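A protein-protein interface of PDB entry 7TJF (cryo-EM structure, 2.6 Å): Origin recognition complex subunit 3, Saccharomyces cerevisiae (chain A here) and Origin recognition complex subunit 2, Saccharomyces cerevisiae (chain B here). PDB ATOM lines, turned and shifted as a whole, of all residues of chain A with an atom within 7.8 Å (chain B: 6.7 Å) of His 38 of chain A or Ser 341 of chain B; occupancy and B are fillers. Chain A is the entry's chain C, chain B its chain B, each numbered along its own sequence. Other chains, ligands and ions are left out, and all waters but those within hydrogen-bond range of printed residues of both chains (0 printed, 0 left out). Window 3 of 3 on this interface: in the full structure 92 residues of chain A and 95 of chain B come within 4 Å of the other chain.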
ATOM      1  N   HIS A  38      17.860  -7.091  13.510  1.00  0.00           N
ATOM      2  CA  HIS A  38      18.751  -7.441  12.411  1.00  0.00           C
ATOM      3  C   HIS A  38      18.229  -8.649  11.640  1.00  0.00           C
ATOM      4  O   HIS A  38      18.949  -9.622  11.434  1.00  0.00           O
ATOM      5  CB  HIS A  38      20.159  -7.723  12.935  1.00  0.00           C
ATOM      6  CG  HIS A  38      21.083  -6.549  12.844  1.00  0.00           C
ATOM      7  ND1 HIS A  38      21.568  -5.895  13.956  1.00  0.00           N
ATOM      8  CD2 HIS A  38      21.606  -5.908  11.771  1.00  0.00           C
ATOM      9  CE1 HIS A  38      22.351  -4.903  13.573  1.00  0.00           C
ATOM     10  NE2 HIS A  38      22.390  -4.888  12.253  1.00  0.00           N
ATOM     11  N   ILE A  39      16.970  -8.578  11.218  1.00  0.00           N
ATOM     12  CA  ILE A  39      16.325  -9.674  10.498  1.00  0.00           C
ATOM     13  C   ILE A  39      15.758  -9.122   9.193  1.00  0.00           C
ATOM     14  O   ILE A  39      15.419  -7.932   9.126  1.00  0.00           O
ATOM     15  CB  ILE A  39      15.241 -10.341  11.362  1.00  0.00           C
ATOM     16  CG1 ILE A  39      14.285  -9.299  11.939  1.00  0.00           C
ATOM     17  CG2 ILE A  39      15.867 -11.175  12.470  1.00  0.00           C
ATOM     18  CD1 ILE A  39      12.920  -9.855  12.246  1.00  0.00           C
ATOM     19  N   PRO A  40      15.652  -9.930   8.129  1.00  0.00           N
ATOM     20  CA  PRO A  40      15.179  -9.396   6.840  1.00  0.00           C
ATOM     21  C   PRO A  40      13.692  -9.091   6.776  1.00  0.00           C
ATOM     22  O   PRO A  40      13.249  -8.555   5.754  1.00  0.00           O
ATOM     23  CB  PRO A  40      15.546 -10.504   5.844  1.00  0.00           C
ATOM     24  CG  PRO A  40      15.705 -11.722   6.657  1.00  0.00           C
ATOM     25  CD  PRO A  40      16.233 -11.274   7.976  1.00  0.00           C
ATOM     26  N   PHE A  41      12.909  -9.419   7.799  1.00  0.00           N
ATOM     27  CA  PHE A  41      11.481  -9.134   7.754  1.00  0.00           C
ATOM     28  C   PHE A  41      11.236  -7.638   7.894  1.00  0.00           C
ATOM     29  O   PHE A  41      11.930  -6.944   8.641  1.00  0.00           O
ATOM     30  CB  PHE A  41      10.745  -9.903   8.851  1.00  0.00           C
ATOM     31  CG  PHE A  41      10.377 -11.313   8.473  1.00  0.00           C
ATOM     32  CD1 PHE A  41      10.842 -11.882   7.297  1.00  0.00           C
ATOM     33  CD2 PHE A  41       9.568 -12.073   9.304  1.00  0.00           C
ATOM     34  CE1 PHE A  41      10.509 -13.174   6.958  1.00  0.00           C
ATOM     35  CE2 PHE A  41       9.227 -13.370   8.966  1.00  0.00           C
ATOM     36  CZ  PHE A  41       9.700 -13.920   7.792  1.00  0.00           C
ATOM     37  N   GLU A  51       7.747  -3.579  15.834  1.00  0.00           N
ATOM     38  CA  GLU A  51       8.909  -4.449  15.664  1.00  0.00           C
ATOM     39  C   GLU A  51       8.760  -5.740  16.465  1.00  0.00           C
ATOM     40  O   GLU A  51       9.355  -6.767  16.105  1.00  0.00           O
ATOM     41  CB  GLU A  51      10.178  -3.690  16.065  1.00  0.00           C
ATOM     42  CG  GLU A  51      11.497  -4.370  15.711  1.00  0.00           C
ATOM     43  CD  GLU A  51      11.770  -4.392  14.218  1.00  0.00           C
ATOM     44  OE1 GLU A  51      11.294  -3.484  13.506  1.00  0.00           O
ATOM     45  OE2 GLU A  51      12.464  -5.322  13.754  1.00  0.00           O
ATOM     46  N   GLU A  55       9.416  -9.442  14.889  1.00  0.00           N
ATOM     47  CA  GLU A  55      10.239 -10.490  15.488  1.00  0.00           C
ATOM     48  C   GLU A  55       9.424 -11.737  15.817  1.00  0.00           C
ATOM     49  O   GLU A  55       9.929 -12.862  15.691  1.00  0.00           O
ATOM     50  CB  GLU A  55      10.933  -9.955  16.741  1.00  0.00           C
ATOM     51  CG  GLU A  55      12.009 -10.873  17.309  1.00  0.00           C
ATOM     52  CD  GLU A  55      13.213 -11.013  16.393  1.00  0.00           C
ATOM     53  OE1 GLU A  55      13.529 -10.048  15.665  1.00  0.00           O
ATOM     54  OE2 GLU A  55      13.844 -12.091  16.401  1.00  0.00           O
ATOM     55  N   TRP A  58       8.981 -13.582  12.646  1.00  0.00           N
ATOM     56  CA  TRP A  58      10.249 -14.249  12.343  1.00  0.00           C
ATOM     57  C   TRP A  58      10.388 -15.560  13.113  1.00  0.00           C
ATOM     58  O   TRP A  58      10.686 -16.616  12.533  1.00  0.00           O
ATOM     59  CB  TRP A  58      11.396 -13.289  12.677  1.00  0.00           C
ATOM     60  CG  TRP A  58      12.773 -13.771  12.355  1.00  0.00           C
ATOM     61  CD1 TRP A  58      13.747 -14.106  13.243  1.00  0.00           C
ATOM     62  CD2 TRP A  58      13.340 -13.942  11.054  1.00  0.00           C
ATOM     63  NE1 TRP A  58      14.884 -14.490  12.579  1.00  0.00           N
ATOM     64  CE2 TRP A  58      14.661 -14.396  11.231  1.00  0.00           C
ATOM     65  CE3 TRP A  58      12.858 -13.761   9.754  1.00  0.00           C
ATOM     66  CZ2 TRP A  58      15.506 -14.670  10.158  1.00  0.00           C
ATOM     67  CZ3 TRP A  58      13.695 -14.038   8.693  1.00  0.00           C
ATOM     68  CH2 TRP A  58      15.003 -14.494   8.901  1.00  0.00           C
ATOM     69  N   TRP B 305      17.692 -10.991   0.717  1.00  0.00           N
ATOM     70  CA  TRP B 305      18.430 -11.462   1.888  1.00  0.00           C
ATOM     71  C   TRP B 305      17.711 -12.634   2.551  1.00  0.00           C
ATOM     72  O   TRP B 305      18.346 -13.627   2.920  1.00  0.00           O
ATOM     73  CB  TRP B 305      18.633 -10.287   2.857  1.00  0.00           C
ATOM     74  CG  TRP B 305      19.255 -10.574   4.216  1.00  0.00           C
ATOM     75  CD1 TRP B 305      20.042 -11.635   4.573  1.00  0.00           C
ATOM     76  CD2 TRP B 305      19.148  -9.751   5.385  1.00  0.00           C
ATOM     77  NE1 TRP B 305      20.406 -11.533   5.890  1.00  0.00           N
ATOM     78  CE2 TRP B 305      19.876 -10.385   6.411  1.00  0.00           C
ATOM     79  CE3 TRP B 305      18.509  -8.539   5.663  1.00  0.00           C
ATOM     80  CZ2 TRP B 305      19.973  -9.853   7.694  1.00  0.00           C
ATOM     81  CZ3 TRP B 305      18.603  -8.016   6.937  1.00  0.00           C
ATOM     82  CH2 TRP B 305      19.331  -8.670   7.935  1.00  0.00           C
ATOM     83  N   THR B 309      19.026 -16.599   3.027  1.00  0.00           N
ATOM     84  CA  THR B 309      19.198 -17.260   4.318  1.00  0.00           C
ATOM     85  C   THR B 309      18.477 -18.599   4.394  1.00  0.00           C
ATOM     86  O   THR B 309      18.805 -19.413   5.261  1.00  0.00           O
ATOM     87  CB  THR B 309      18.718 -16.362   5.462  1.00  0.00           C
ATOM     88  OG1 THR B 309      17.356 -15.974   5.241  1.00  0.00           O
ATOM     89  CG2 THR B 309      19.592 -15.127   5.583  1.00  0.00           C
ATOM     90  N   PRO B 336      27.232  -6.636   5.110  1.00  0.00           N
ATOM     91  CA  PRO B 336      27.034  -6.134   6.483  1.00  0.00           C
ATOM     92  C   PRO B 336      25.821  -6.709   7.197  1.00  0.00           C
ATOM     93  O   PRO B 336      25.891  -6.906   8.414  1.00  0.00           O
ATOM     94  CB  PRO B 336      26.895  -4.618   6.289  1.00  0.00           C
ATOM     95  CG  PRO B 336      27.604  -4.343   5.053  1.00  0.00           C
ATOM     96  CD  PRO B 336      27.288  -5.493   4.173  1.00  0.00           C
ATOM     97  N   LYS B 337      24.725  -6.999   6.486  1.00  0.00           N
ATOM     98  CA  LYS B 337      23.557  -7.590   7.136  1.00  0.00           C
ATOM     99  C   LYS B 337      23.847  -9.001   7.630  1.00  0.00           C
ATOM    100  O   LYS B 337      23.459  -9.363   8.750  1.00  0.00           O
ATOM    101  CB  LYS B 337      22.361  -7.599   6.183  1.00  0.00           C
ATOM    102  CG  LYS B 337      21.843  -6.227   5.790  1.00  0.00           C
ATOM    103  CD  LYS B 337      21.241  -5.486   6.961  1.00  0.00           C
ATOM    104  CE  LYS B 337      20.933  -4.047   6.584  1.00  0.00           C
ATOM    105  NZ  LYS B 337      19.862  -3.472   7.444  1.00  0.00           N
ATOM    106  N   ILE B 338      24.540  -9.803   6.816  1.00  0.00           N
ATOM    107  CA  ILE B 338      24.905 -11.157   7.223  1.00  0.00           C
ATOM    108  C   ILE B 338      25.909 -11.119   8.372  1.00  0.00           C
ATOM    109  O   ILE B 338      25.798 -11.892   9.333  1.00  0.00           O
ATOM    110  CB  ILE B 338      25.438 -11.947   6.009  1.00  0.00           C
ATOM    111  CG1 ILE B 338      24.316 -12.175   4.996  1.00  0.00           C
ATOM    112  CG2 ILE B 338      26.027 -13.292   6.428  1.00  0.00           C
ATOM    113  CD1 ILE B 338      24.719 -12.996   3.799  1.00  0.00           C
ATOM    114  N   ALA B 339      26.874 -10.193   8.314  1.00  0.00           N
ATOM    115  CA  ALA B 339      27.890 -10.107   9.360  1.00  0.00           C
ATOM    116  C   ALA B 339      27.309  -9.614  10.683  1.00  0.00           C
ATOM    117  O   ALA B 339      27.688 -10.111  11.750  1.00  0.00           O
ATOM    118  CB  ALA B 339      29.032  -9.201   8.904  1.00  0.00           C
ATOM    119  N   TYR B 340      26.389  -8.647  10.641  1.00  0.00           N
ATOM    120  CA  TYR B 340      25.782  -8.154  11.872  1.00  0.00           C
ATOM    121  C   TYR B 340      24.766  -9.139  12.435  1.00  0.00           C
ATOM    122  O   TYR B 340      24.609  -9.227  13.658  1.00  0.00           O
ATOM    123  CB  TYR B 340      25.124  -6.796  11.636  1.00  0.00           C
ATOM    124  CG  TYR B 340      26.097  -5.653  11.455  1.00  0.00           C
ATOM    125  CD1 TYR B 340      27.319  -5.642  12.118  1.00  0.00           C
ATOM    126  CD2 TYR B 340      25.791  -4.580  10.624  1.00  0.00           C
ATOM    127  CE1 TYR B 340      28.214  -4.596  11.953  1.00  0.00           C
ATOM    128  CE2 TYR B 340      26.675  -3.532  10.451  1.00  0.00           C
ATOM    129  CZ  TYR B 340      27.884  -3.544  11.118  1.00  0.00           C
ATOM    130  OH  TYR B 340      28.765  -2.502  10.950  1.00  0.00           O
ATOM    131  N   SER B 341      24.071  -9.886  11.574  1.00  0.00           N
ATOM    132  CA  SER B 341      23.116 -10.872  12.065  1.00  0.00           C
ATOM    133  C   SER B 341      23.788 -12.115  12.635  1.00  0.00           C
ATOM    134  O   SER B 341      23.125 -12.893  13.326  1.00  0.00           O
ATOM    135  CB  SER B 341      22.151 -11.271  10.946  1.00  0.00           C
ATOM    136  OG  SER B 341      22.827 -11.939   9.900  1.00  0.00           O
ATOM    137  N   GLN B 342      25.078 -12.319  12.367  1.00  0.00           N
ATOM    138  CA  GLN B 342      25.810 -13.486  12.840  1.00  0.00           C
ATOM    139  C   GLN B 342      26.682 -13.173  14.051  1.00  0.00           C
ATOM    140  O   GLN B 342      27.701 -13.836  14.270  1.00  0.00           O
ATOM    141  CB  GLN B 342      26.662 -14.069  11.711  1.00  0.00           C
ATOM    142  CG  GLN B 342      25.909 -14.998  10.775  1.00  0.00           C
ATOM    143  CD  GLN B 342      26.675 -15.286   9.497  1.00  0.00           C
ATOM    144  OE1 GLN B 342      26.147 -15.898   8.572  1.00  0.00           O
ATOM    145  NE2 GLN B 342      27.923 -14.839   9.439  1.00  0.00           N
ATOM    146  N   LEU B 343      26.306 -12.171  14.840  1.00  0.00           N
ATOM    147  CA  LEU B 343      27.048 -11.837  16.049  1.00  0.00           C
ATOM    148  C   LEU B 343      26.534 -12.642  17.239  1.00  0.00           C
ATOM    149  O   LEU B 343      27.184 -13.581  17.694  1.00  0.00           O
ATOM    150  CB  LEU B 343      26.951 -10.341  16.345  1.00  0.00           C
ATOM    151  CG  LEU B 343      27.597  -9.389  15.335  1.00  0.00           C
ATOM    152  CD1 LEU B 343      27.431  -7.948  15.783  1.00  0.00           C
ATOM    153  CD2 LEU B 343      29.064  -9.726  15.132  1.00  0.00           C
ATOM    154  N   ASP B 417      25.732 -20.771   9.127  1.00  0.00           N
ATOM    155  CA  ASP B 417      26.111 -19.368   9.062  1.00  0.00           C
ATOM    156  C   ASP B 417      26.907 -19.133   7.788  1.00  0.00           C
ATOM    157  O   ASP B 417      27.849 -19.877   7.498  1.00  0.00           O
ATOM    158  CB  ASP B 417      26.933 -18.963  10.287  1.00  0.00           C
ATOM    159  CG  ASP B 417      26.090 -18.841  11.538  1.00  0.00           C
ATOM    160  OD1 ASP B 417      25.156 -19.652  11.709  1.00  0.00           O
ATOM    161  OD2 ASP B 417      26.358 -17.930  12.351  1.00  0.00           O
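OG of Ser 341 of chain B is in hydrogen-bond range of O of Ile 338 of chain B (3.0 Å). The backbone carbonyl oxygen (O) of Lys 337 of chain B lies within hydrogen-bond range of the side-chain hydroxyl (OG) of Ser 341 of chain B. The side-chain hydroxyl of Thr 309 of chain B lies close to the backbone carbonyl oxygen of Trp 305 of chain B (3.4 Å).
Of chain B, only Trp 305 (3.6 Å), Tyr 340 (3.4 Å) and Ser 341 (3.6 Å) come within 4 Å of His 38 of chain A. Printed residues of chain B within 4 Å of Ile 39 of chain A: Trp 305. Of the printed residues of chain B, Pro 40 of chain A touches Trp 305. Phe 41 of chain A touches none of the printed residues of chain B. Of the printed residues of chain A, Trp 305 of chain B touches His 38, Ile 39 and Pro 40. Of chain A, only His 38 (3.6 Å) comes within 4 Å of Ser 341 of chain B. Leu 343 of chain B touches none of the printed residues of chain A. The nearest residue of chain B that does not touch His 38 of chain A is Lys 337 of chain B (4.8 Å). The nearest residue of chain A that does not touch Ser 341 of chain B is Ile 39 of chain A (5.8 Å).
Among the printed residues, pairs that only touch across the chains: His 38 of chain A with Trp 305 of chain B (3.6 Å), His 38 of chain A with Tyr 340 of chain B (3.4 Å), His 38 of chain A with Ser 341 of chain B (3.6 Å), Ile 39 of chain A with Trp 305 of chain B (3.8 Å) and Pro 40 of chain A with Trp 305 of chain B (3.6 Å).
Hydrophobic or aromatic side chains of chain B within 4 Å of the printed part of chain A: Trp 305 and Tyr 340. Along chain B the printed residues that touch a printed residue of chain A span positions 305 to 341. Among the printed residues, no Asp or Glu carboxylate lies within 4 Å of a Lys or Arg side-chain nitrogen of the other chain.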
